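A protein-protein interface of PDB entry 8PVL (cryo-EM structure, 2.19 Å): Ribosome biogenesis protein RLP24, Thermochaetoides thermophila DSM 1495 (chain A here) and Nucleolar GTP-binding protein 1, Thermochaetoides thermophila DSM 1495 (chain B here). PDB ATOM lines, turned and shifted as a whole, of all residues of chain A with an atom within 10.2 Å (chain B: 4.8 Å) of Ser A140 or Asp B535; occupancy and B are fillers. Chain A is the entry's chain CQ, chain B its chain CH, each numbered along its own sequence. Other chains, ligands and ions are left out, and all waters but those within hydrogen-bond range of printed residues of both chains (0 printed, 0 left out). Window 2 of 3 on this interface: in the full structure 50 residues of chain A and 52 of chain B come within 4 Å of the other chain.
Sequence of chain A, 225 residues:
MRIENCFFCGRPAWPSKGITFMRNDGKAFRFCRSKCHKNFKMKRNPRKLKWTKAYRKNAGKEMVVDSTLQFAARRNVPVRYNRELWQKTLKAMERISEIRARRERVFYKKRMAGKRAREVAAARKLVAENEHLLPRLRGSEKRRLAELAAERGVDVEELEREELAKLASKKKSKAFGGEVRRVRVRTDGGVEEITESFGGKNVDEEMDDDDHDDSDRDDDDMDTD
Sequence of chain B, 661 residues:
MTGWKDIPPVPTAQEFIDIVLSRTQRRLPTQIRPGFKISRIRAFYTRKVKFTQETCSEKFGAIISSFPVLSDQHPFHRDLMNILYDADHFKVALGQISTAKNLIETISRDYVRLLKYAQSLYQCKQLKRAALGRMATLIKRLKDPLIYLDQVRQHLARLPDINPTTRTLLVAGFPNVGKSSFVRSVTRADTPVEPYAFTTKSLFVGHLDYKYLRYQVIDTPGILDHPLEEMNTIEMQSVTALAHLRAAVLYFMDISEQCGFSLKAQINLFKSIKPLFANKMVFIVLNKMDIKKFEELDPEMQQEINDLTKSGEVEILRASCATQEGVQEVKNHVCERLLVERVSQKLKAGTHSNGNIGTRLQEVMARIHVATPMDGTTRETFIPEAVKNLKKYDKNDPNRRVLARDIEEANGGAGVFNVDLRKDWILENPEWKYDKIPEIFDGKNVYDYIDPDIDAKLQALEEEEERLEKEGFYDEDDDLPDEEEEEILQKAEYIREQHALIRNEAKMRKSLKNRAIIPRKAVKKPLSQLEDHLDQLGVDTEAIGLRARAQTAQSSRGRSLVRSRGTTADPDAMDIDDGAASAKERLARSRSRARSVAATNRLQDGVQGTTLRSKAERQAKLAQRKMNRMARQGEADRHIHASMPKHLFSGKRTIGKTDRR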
ATOM      1  N   PRO A 135     -11.200  -7.053 -24.672  1.00  0.00           N
ATOM      2  CA  PRO A 135     -11.649  -7.934 -23.583  1.00  0.00           C
ATOM      3  C   PRO A 135     -13.153  -7.865 -23.367  1.00  0.00           C
ATOM      4  O   PRO A 135     -13.762  -6.795 -23.416  1.00  0.00           O
ATOM      5  CB  PRO A 135     -10.887  -7.412 -22.360  1.00  0.00           C
ATOM      6  CG  PRO A 135     -10.522  -6.023 -22.698  1.00  0.00           C
ATOM      7  CD  PRO A 135     -10.292  -6.004 -24.171  1.00  0.00           C
ATOM      8  N   ARG A 136     -13.743  -9.031 -23.123  1.00  0.00           N
ATOM      9  CA  ARG A 136     -15.180  -9.168 -22.959  1.00  0.00           C
ATOM     10  C   ARG A 136     -15.454 -10.166 -21.847  1.00  0.00           C
ATOM     11  O   ARG A 136     -14.555 -10.857 -21.364  1.00  0.00           O
ATOM     12  CB  ARG A 136     -15.854  -9.623 -24.258  1.00  0.00           C
ATOM     13  CG  ARG A 136     -15.460 -11.028 -24.687  1.00  0.00           C
ATOM     14  CD  ARG A 136     -15.879 -11.315 -26.116  1.00  0.00           C
ATOM     15  NE  ARG A 136     -15.921 -10.107 -26.929  1.00  0.00           N
ATOM     16  CZ  ARG A 136     -16.256 -10.079 -28.211  1.00  0.00           C
ATOM     17  NH1 ARG A 136     -16.584 -11.181 -28.864  1.00  0.00           N
ATOM     18  NH2 ARG A 136     -16.260  -8.915 -28.856  1.00  0.00           N
ATOM     19  N   LEU A 137     -16.716 -10.238 -21.444  1.00  0.00           N
ATOM     20  CA  LEU A 137     -17.141 -11.192 -20.435  1.00  0.00           C
ATOM     21  C   LEU A 137     -17.548 -12.507 -21.084  1.00  0.00           C
ATOM     22  O   LEU A 137     -17.966 -12.549 -22.245  1.00  0.00           O
ATOM     23  CB  LEU A 137     -18.305 -10.634 -19.618  1.00  0.00           C
ATOM     24  CG  LEU A 137     -17.988  -9.380 -18.806  1.00  0.00           C
ATOM     25  CD1 LEU A 137     -19.258  -8.623 -18.495  1.00  0.00           C
ATOM     26  CD2 LEU A 137     -17.254  -9.749 -17.531  1.00  0.00           C
ATOM     27  N   ARG A 138     -17.416 -13.586 -20.319  1.00  0.00           N
ATOM     28  CA  ARG A 138     -17.862 -14.888 -20.779  1.00  0.00           C
ATOM     29  C   ARG A 138     -19.386 -14.938 -20.834  1.00  0.00           C
ATOM     30  O   ARG A 138     -20.082 -14.127 -20.219  1.00  0.00           O
ATOM     31  CB  ARG A 138     -17.334 -15.990 -19.860  1.00  0.00           C
ATOM     32  CG  ARG A 138     -15.852 -16.281 -20.018  1.00  0.00           C
ATOM     33  CD  ARG A 138     -15.343 -17.146 -18.879  1.00  0.00           C
ATOM     34  NE  ARG A 138     -14.010 -17.677 -19.136  1.00  0.00           N
ATOM     35  CZ  ARG A 138     -13.764 -18.891 -19.609  1.00  0.00           C
ATOM     36  NH1 ARG A 138     -14.744 -19.729 -19.906  1.00  0.00           N
ATOM     37  NH2 ARG A 138     -12.504 -19.275 -19.789  1.00  0.00           N
ATOM     38  N   GLY A 139     -19.903 -15.900 -21.601  1.00  0.00           N
ATOM     39  CA  GLY A 139     -21.342 -16.103 -21.638  1.00  0.00           C
ATOM     40  C   GLY A 139     -21.897 -16.567 -20.305  1.00  0.00           C
ATOM     41  O   GLY A 139     -22.953 -16.104 -19.864  1.00  0.00           O
ATOM     42  N   SER A 140     -21.182 -17.475 -19.637  1.00  0.00           N
ATOM     43  CA  SER A 140     -21.584 -17.918 -18.306  1.00  0.00           C
ATOM     44  C   SER A 140     -21.487 -16.785 -17.292  1.00  0.00           C
ATOM     45  O   SER A 140     -22.337 -16.665 -16.401  1.00  0.00           O
ATOM     46  CB  SER A 140     -20.727 -19.104 -17.873  1.00  0.00           C
ATOM     47  OG  SER A 140     -19.358 -18.742 -17.817  1.00  0.00           O
ATOM     48  N   GLU A 141     -20.451 -15.948 -17.411  1.00  0.00           N
ATOM     49  CA  GLU A 141     -20.321 -14.791 -16.531  1.00  0.00           C
ATOM     50  C   GLU A 141     -21.459 -13.802 -16.747  1.00  0.00           C
ATOM     51  O   GLU A 141     -21.997 -13.250 -15.783  1.00  0.00           O
ATOM     52  CB  GLU A 141     -18.971 -14.110 -16.753  1.00  0.00           C
ATOM     53  CG  GLU A 141     -17.826 -14.720 -15.962  1.00  0.00           C
ATOM     54  CD  GLU A 141     -18.182 -14.959 -14.508  1.00  0.00           C
ATOM     55  OE1 GLU A 141     -18.190 -13.982 -13.731  1.00  0.00           O
ATOM     56  OE2 GLU A 141     -18.443 -16.124 -14.139  1.00  0.00           O
ATOM     57  N   LYS A 142     -21.845 -13.579 -18.006  1.00  0.00           N
ATOM     58  CA  LYS A 142     -22.974 -12.702 -18.297  1.00  0.00           C
ATOM     59  C   LYS A 142     -24.280 -13.282 -17.769  1.00  0.00           C
ATOM     60  O   LYS A 142     -25.133 -12.541 -17.270  1.00  0.00           O
ATOM     61  CB  LYS A 142     -23.071 -12.448 -19.800  1.00  0.00           C
ATOM     62  CG  LYS A 142     -22.559 -11.086 -20.233  1.00  0.00           C
ATOM     63  CD  LYS A 142     -21.741 -11.190 -21.506  1.00  0.00           C
ATOM     64  CE  LYS A 142     -22.632 -11.449 -22.709  1.00  0.00           C
ATOM     65  NZ  LYS A 142     -21.881 -12.092 -23.821  1.00  0.00           N
ATOM     66  N   ARG A 143     -24.450 -14.605 -17.864  1.00  0.00           N
ATOM     67  CA  ARG A 143     -25.641 -15.254 -17.317  1.00  0.00           C
ATOM     68  C   ARG A 143     -25.718 -15.091 -15.802  1.00  0.00           C
ATOM     69  O   ARG A 143     -26.776 -14.754 -15.249  1.00  0.00           O
ATOM     70  CB  ARG A 143     -25.640 -16.737 -17.687  1.00  0.00           C
ATOM     71  CG  ARG A 143     -26.466 -17.093 -18.907  1.00  0.00           C
ATOM     72  CD  ARG A 143     -26.998 -18.519 -18.812  1.00  0.00           C
ATOM     73  NE  ARG A 143     -26.073 -19.429 -18.143  1.00  0.00           N
ATOM     74  CZ  ARG A 143     -25.012 -19.983 -18.715  1.00  0.00           C
ATOM     75  NH1 ARG A 143     -24.707 -19.750 -19.981  1.00  0.00           N
ATOM     76  NH2 ARG A 143     -24.239 -20.796 -18.000  1.00  0.00           N
ATOM     77  N   ARG A 144     -24.595 -15.318 -15.112  1.00  0.00           N
ATOM     78  CA  ARG A 144     -24.606 -15.210 -13.658  1.00  0.00           C
ATOM     79  C   ARG A 144     -24.746 -13.759 -13.206  1.00  0.00           C
ATOM     80  O   ARG A 144     -25.393 -13.496 -12.189  1.00  0.00           O
ATOM     81  CB  ARG A 144     -23.360 -15.877 -13.055  1.00  0.00           C
ATOM     82  CG  ARG A 144     -22.123 -15.001 -12.898  1.00  0.00           C
ATOM     83  CD  ARG A 144     -21.245 -15.486 -11.755  1.00  0.00           C
ATOM     84  NE  ARG A 144     -20.223 -14.509 -11.399  1.00  0.00           N
ATOM     85  CZ  ARG A 144     -19.353 -14.664 -10.411  1.00  0.00           C
ATOM     86  NH1 ARG A 144     -19.355 -15.747  -9.652  1.00  0.00           N
ATOM     87  NH2 ARG A 144     -18.458 -13.708 -10.178  1.00  0.00           N
ATOM     88  N   LEU A 145     -24.214 -12.802 -13.974  1.00  0.00           N
ATOM     89  CA  LEU A 145     -24.416 -11.400 -13.630  1.00  0.00           C
ATOM     90  C   LEU A 145     -25.845 -10.961 -13.905  1.00  0.00           C
ATOM     91  O   LEU A 145     -26.388 -10.136 -13.164  1.00  0.00           O
ATOM     92  CB  LEU A 145     -23.428 -10.517 -14.391  1.00  0.00           C
ATOM     93  CG  LEU A 145     -21.979 -10.539 -13.898  1.00  0.00           C
ATOM     94  CD1 LEU A 145     -21.142  -9.491 -14.617  1.00  0.00           C
ATOM     95  CD2 LEU A 145     -21.917 -10.342 -12.393  1.00  0.00           C
ATOM     96  N   ALA A 146     -26.476 -11.514 -14.944  1.00  0.00           N
ATOM     97  CA  ALA A 146     -27.881 -11.223 -15.199  1.00  0.00           C
ATOM     98  C   ALA A 146     -28.771 -11.752 -14.079  1.00  0.00           C
ATOM     99  O   ALA A 146     -29.704 -11.064 -13.647  1.00  0.00           O
ATOM    100  CB  ALA A 146     -28.297 -11.802 -16.552  1.00  0.00           C
ATOM    101  N   GLU A 147     -28.495 -12.962 -13.578  1.00  0.00           N
ATOM    102  CA  GLU A 147     -29.349 -13.486 -12.512  1.00  0.00           C
ATOM    103  C   GLU A 147     -29.031 -12.860 -11.150  1.00  0.00           C
ATOM    104  O   GLU A 147     -29.941 -12.702 -10.329  1.00  0.00           O
ATOM    105  CB  GLU A 147     -29.315 -15.023 -12.507  1.00  0.00           C
ATOM    106  CG  GLU A 147     -27.990 -15.746 -12.303  1.00  0.00           C
ATOM    107  CD  GLU A 147     -27.565 -15.889 -10.863  1.00  0.00           C
ATOM    108  OE1 GLU A 147     -26.401 -16.286 -10.645  1.00  0.00           O
ATOM    109  OE2 GLU A 147     -28.379 -15.624  -9.955  1.00  0.00           O
ATOM    110  N   LEU A 148     -27.780 -12.434 -10.914  1.00  0.00           N
ATOM    111  CA  LEU A 148     -27.506 -11.552  -9.776  1.00  0.00           C
ATOM    112  C   LEU A 148     -28.243 -10.222  -9.888  1.00  0.00           C
ATOM    113  O   LEU A 148     -28.733  -9.704  -8.878  1.00  0.00           O
ATOM    114  CB  LEU A 148     -26.005 -11.286  -9.605  1.00  0.00           C
ATOM    115  CG  LEU A 148     -25.038 -12.201  -8.842  1.00  0.00           C
ATOM    116  CD1 LEU A 148     -25.077 -11.815  -7.380  1.00  0.00           C
ATOM    117  CD2 LEU A 148     -25.345 -13.671  -8.951  1.00  0.00           C
ATOM    118  N   GLU A 160     -21.639  -5.714 -14.897  1.00  0.00           N
ATOM    119  CA  GLU A 160     -20.799  -6.016 -16.050  1.00  0.00           C
ATOM    120  C   GLU A 160     -19.539  -5.155 -16.068  1.00  0.00           C
ATOM    121  O   GLU A 160     -18.438  -5.665 -16.316  1.00  0.00           O
ATOM    122  CB  GLU A 160     -21.604  -5.829 -17.336  1.00  0.00           C
ATOM    123  CG  GLU A 160     -22.464  -7.031 -17.705  1.00  0.00           C
ATOM    124  CD  GLU A 160     -23.442  -6.723 -18.819  1.00  0.00           C
ATOM    125  OE1 GLU A 160     -23.576  -5.535 -19.181  1.00  0.00           O
ATOM    126  OE2 GLU A 160     -24.079  -7.667 -19.333  1.00  0.00           O
ATOM    127  N   GLU A 163     -17.187  -6.348 -13.212  1.00  0.00           N
ATOM    128  CA  GLU A 163     -16.502  -7.595 -13.537  1.00  0.00           C
ATOM    129  C   GLU A 163     -15.468  -7.392 -14.637  1.00  0.00           C
ATOM    130  O   GLU A 163     -14.423  -8.049 -14.628  1.00  0.00           O
ATOM    131  CB  GLU A 163     -17.525  -8.660 -13.948  1.00  0.00           C
ATOM    132  CG  GLU A 163     -17.629  -9.956 -13.083  1.00  0.00           C
ATOM    133  CD  GLU A 163     -16.365 -10.826 -12.937  1.00  0.00           C
ATOM    134  OE1 GLU A 163     -16.513 -11.977 -12.471  1.00  0.00           O
ATOM    135  OE2 GLU A 163     -15.244 -10.420 -13.302  1.00  0.00           O
ATOM    136  N   LEU A 167     -11.593  -8.245 -14.221  1.00  0.00           N
ATOM    137  CA  LEU A 167     -10.902  -9.075 -15.203  1.00  0.00           C
ATOM    138  C   LEU A 167      -9.692  -8.355 -15.785  1.00  0.00           C
ATOM    139  O   LEU A 167      -8.683  -8.990 -16.108  1.00  0.00           O
ATOM    140  CB  LEU A 167     -11.868  -9.481 -16.315  1.00  0.00           C
ATOM    141  CG  LEU A 167     -12.682 -10.762 -16.116  1.00  0.00           C
ATOM    142  CD1 LEU A 167     -13.235 -11.249 -17.446  1.00  0.00           C
ATOM    143  CD2 LEU A 167     -11.848 -11.849 -15.452  1.00  0.00           C
ATOM    144  N   GLU B 531     -16.839 -25.819 -25.832  1.00  0.00           N
ATOM    145  CA  GLU B 531     -17.632 -25.025 -24.902  1.00  0.00           C
ATOM    146  C   GLU B 531     -16.804 -23.909 -24.282  1.00  0.00           C
ATOM    147  O   GLU B 531     -17.280 -22.776 -24.155  1.00  0.00           O
ATOM    148  CB  GLU B 531     -18.205 -25.927 -23.808  1.00  0.00           C
ATOM    149  CG  GLU B 531     -19.711 -26.104 -23.854  1.00  0.00           C
ATOM    150  CD  GLU B 531     -20.184 -27.236 -22.962  1.00  0.00           C
ATOM    151  OE1 GLU B 531     -19.505 -27.525 -21.955  1.00  0.00           O
ATOM    152  OE2 GLU B 531     -21.235 -27.839 -23.269  1.00  0.00           O
ATOM    153  N   ASP B 532     -15.559 -24.211 -23.900  1.00  0.00           N
ATOM    154  CA  ASP B 532     -14.692 -23.199 -23.305  1.00  0.00           C
ATOM    155  C   ASP B 532     -14.359 -22.096 -24.300  1.00  0.00           C
ATOM    156  O   ASP B 532     -14.367 -20.912 -23.945  1.00  0.00           O
ATOM    157  CB  ASP B 532     -13.414 -23.852 -22.782  1.00  0.00           C
ATOM    158  CG  ASP B 532     -12.556 -22.893 -21.982  1.00  0.00           C
ATOM    159  OD1 ASP B 532     -13.105 -21.916 -21.433  1.00  0.00           O
ATOM    160  OD2 ASP B 532     -11.330 -23.117 -21.904  1.00  0.00           O
ATOM    161  N   HIS B 533     -14.079 -22.461 -25.556  1.00  0.00           N
ATOM    162  CA  HIS B 533     -13.746 -21.446 -26.552  1.00  0.00           C
ATOM    163  C   HIS B 533     -14.952 -20.574 -26.885  1.00  0.00           C
ATOM    164  O   HIS B 533     -14.819 -19.352 -27.019  1.00  0.00           O
ATOM    165  CB  HIS B 533     -13.193 -22.097 -27.817  1.00  0.00           C
ATOM    166  CG  HIS B 533     -12.700 -21.111 -28.829  1.00  0.00           C
ATOM    167  ND1 HIS B 533     -11.436 -20.566 -28.779  1.00  0.00           N
ATOM    168  CD2 HIS B 533     -13.308 -20.555 -29.903  1.00  0.00           C
ATOM    169  CE1 HIS B 533     -11.280 -19.727 -29.787  1.00  0.00           C
ATOM    170  NE2 HIS B 533     -12.402 -19.701 -30.484  1.00  0.00           N
ATOM    171  N   LEU B 534     -16.139 -21.180 -27.008  1.00  0.00           N
ATOM    172  CA  LEU B 534     -17.340 -20.388 -27.262  1.00  0.00           C
ATOM    173  C   LEU B 534     -17.676 -19.488 -26.075  1.00  0.00           C
ATOM    174  O   LEU B 534     -18.129 -18.351 -26.260  1.00  0.00           O
ATOM    175  CB  LEU B 534     -18.512 -21.307 -27.597  1.00  0.00           C
ATOM    176  CG  LEU B 534     -18.437 -21.991 -28.963  1.00  0.00           C
ATOM    177  CD1 LEU B 534     -19.679 -22.826 -29.211  1.00  0.00           C
ATOM    178  CD2 LEU B 534     -18.245 -20.968 -30.071  1.00  0.00           C
ATOM    179  N   ASP B 535     -17.450 -19.979 -24.853  1.00  0.00           N
ATOM    180  CA  ASP B 535     -17.676 -19.164 -23.665  1.00  0.00           C
ATOM    181  C   ASP B 535     -16.719 -17.980 -23.614  1.00  0.00           C
ATOM    182  O   ASP B 535     -17.119 -16.867 -23.258  1.00  0.00           O
ATOM    183  CB  ASP B 535     -17.534 -20.024 -22.410  1.00  0.00           C
ATOM    184  CG  ASP B 535     -18.043 -19.329 -21.166  1.00  0.00           C
ATOM    185  OD1 ASP B 535     -18.986 -18.519 -21.278  1.00  0.00           O
ATOM    186  OD2 ASP B 535     -17.498 -19.594 -20.073  1.00  0.00           O
ATOM    187  N   GLN B 536     -15.447 -18.202 -23.965  1.00  0.00           N
ATOM    188  CA  GLN B 536     -14.499 -17.094 -24.038  1.00  0.00           C
ATOM    189  C   GLN B 536     -14.867 -16.108 -25.136  1.00  0.00           C
ATOM    190  O   GLN B 536     -14.655 -14.901 -24.979  1.00  0.00           O
ATOM    191  CB  GLN B 536     -13.079 -17.618 -24.256  1.00  0.00           C
ATOM    192  CG  GLN B 536     -12.514 -18.387 -23.080  1.00  0.00           C
ATOM    193  CD  GLN B 536     -11.094 -17.981 -22.750  1.00  0.00           C
ATOM    194  OE1 GLN B 536     -10.200 -18.824 -22.660  1.00  0.00           O
ATOM    195  NE2 GLN B 536     -10.876 -16.685 -22.565  1.00  0.00           N
ATOM    196  N   LEU B 537     -15.417 -16.596 -26.250  1.00  0.00           N
ATOM    197  CA  LEU B 537     -15.902 -15.694 -27.288  1.00  0.00           C
ATOM    198  C   LEU B 537     -17.159 -14.949 -26.864  1.00  0.00           C
ATOM    199  O   LEU B 537     -17.479 -13.914 -27.457  1.00  0.00           O
ATOM    200  CB  LEU B 537     -16.167 -16.466 -28.579  1.00  0.00           C
ATOM    201  CG  LEU B 537     -14.929 -16.959 -29.325  1.00  0.00           C
ATOM    202  CD1 LEU B 537     -15.331 -17.641 -30.614  1.00  0.00           C
ATOM    203  CD2 LEU B 537     -13.980 -15.808 -29.601  1.00  0.00           C
ATOM    204  N   GLY B 538     -17.878 -15.450 -25.868  1.00  0.00           N
ATOM    205  CA  GLY B 538     -19.040 -14.773 -25.346  1.00  0.00           C
ATOM    206  C   GLY B 538     -20.368 -15.310 -25.820  1.00  0.00           C
ATOM    207  O   GLY B 538     -21.327 -14.538 -25.920  1.00  0.00           O
ATOM    208  N   VAL B 539     -20.457 -16.603 -26.113  1.00  0.00           N
ATOM    209  CA  VAL B 539     -21.678 -17.225 -26.603  1.00  0.00           C
ATOM    210  C   VAL B 539     -22.286 -18.042 -25.474  1.00  0.00           C
ATOM    211  O   VAL B 539     -21.586 -18.824 -24.818  1.00  0.00           O
ATOM    212  CB  VAL B 539     -21.395 -18.104 -27.834  1.00  0.00           C
ATOM    213  CG1 VAL B 539     -22.673 -18.754 -28.339  1.00  0.00           C
ATOM    214  CG2 VAL B 539     -20.742 -17.281 -28.931  1.00  0.00           C
ATOM    215  N   THR B 541     -23.583 -20.970 -24.340  1.00  0.00           N
ATOM    216  CA  THR B 541     -23.612 -22.344 -24.831  1.00  0.00           C
ATOM    217  C   THR B 541     -24.805 -23.116 -24.283  1.00  0.00           C
ATOM    218  O   THR B 541     -25.314 -24.026 -24.951  1.00  0.00           O
ATOM    219  CB  THR B 541     -22.308 -23.056 -24.472  1.00  0.00           C
ATOM    220  OG1 THR B 541     -22.186 -23.141 -23.047  1.00  0.00           O
ATOM    221  CG2 THR B 541     -21.117 -22.293 -25.031  1.00  0.00           C
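O of Gly B538 is in hydrogen-bond range of NZ of Lys A142 (3.3 Å).
NH1 of Arg A138 is in salt-bridge range of OD2 of Asp B535 (2.8 Å).
The side-chain carboxylate of Asp B535 sits at hydrogen-bond distance from the backbone NH of Gly A139 (2.8 Å).
The backbone carbonyl oxygen of Leu B537 is in hydrogen-bond range of the guanidinium group of Arg A136, at 3.2 Å.
The side-chain carboxylate (OD1) of Asp B535 sits at hydrogen-bond distance from the backbone NH (N) of Ser A140, at 2.9 Å.
The guanidinium group (NH1) of Arg A138 lies within salt-bridge range of the side-chain carboxylate (OD1) of Asp B532, 3.1 Å away.
Of chain B, only Asp B535 comes within 4 Å of Ser A140.
Of the printed residues of chain A, Asp B535 touches Arg A138, Gly A139 and Ser A140.
No residue of chain A comes within 4 Å of Leu B534.
Of the printed residues of chain A, Leu B537 touches Arg A136.
Of the printed residues of chain A, Gly B538 touches Leu A137 and Lys A142.
Of the printed residues of chain B, Arg A136 touches Gln B536 (3.96 Å) and Leu B537 (3.2 Å).
Of the printed residues of chain B, Leu A137 touches Gly B538.
Of the printed residues of chain B, Arg A138 touches Asp B532, Asp B535 and Gln B536.
Arg A143 touches none of the printed residues of chain B.
The nearest residue of chain A that does not touch Asp B535 is Leu A137 (4.5 Å).
Among the printed residues, pairs that only touch across the chains: Arg A138 with Gln B536, Arg A136 with Gln B536 and Leu A137 with Gly B538.
Of the 10 printed residues of chain B, 5 touch a printed residue of chain A.
Among the printed residues, 9 pairs touch across the chains.
Among the printed residues, Asp or Glu carboxylates within 4 Å of a Lys or Arg side-chain nitrogen of the other chain: Arg A138 with Asp B532 (3.1 Å) and Arg A138 with Asp B535 (2.8 Å).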
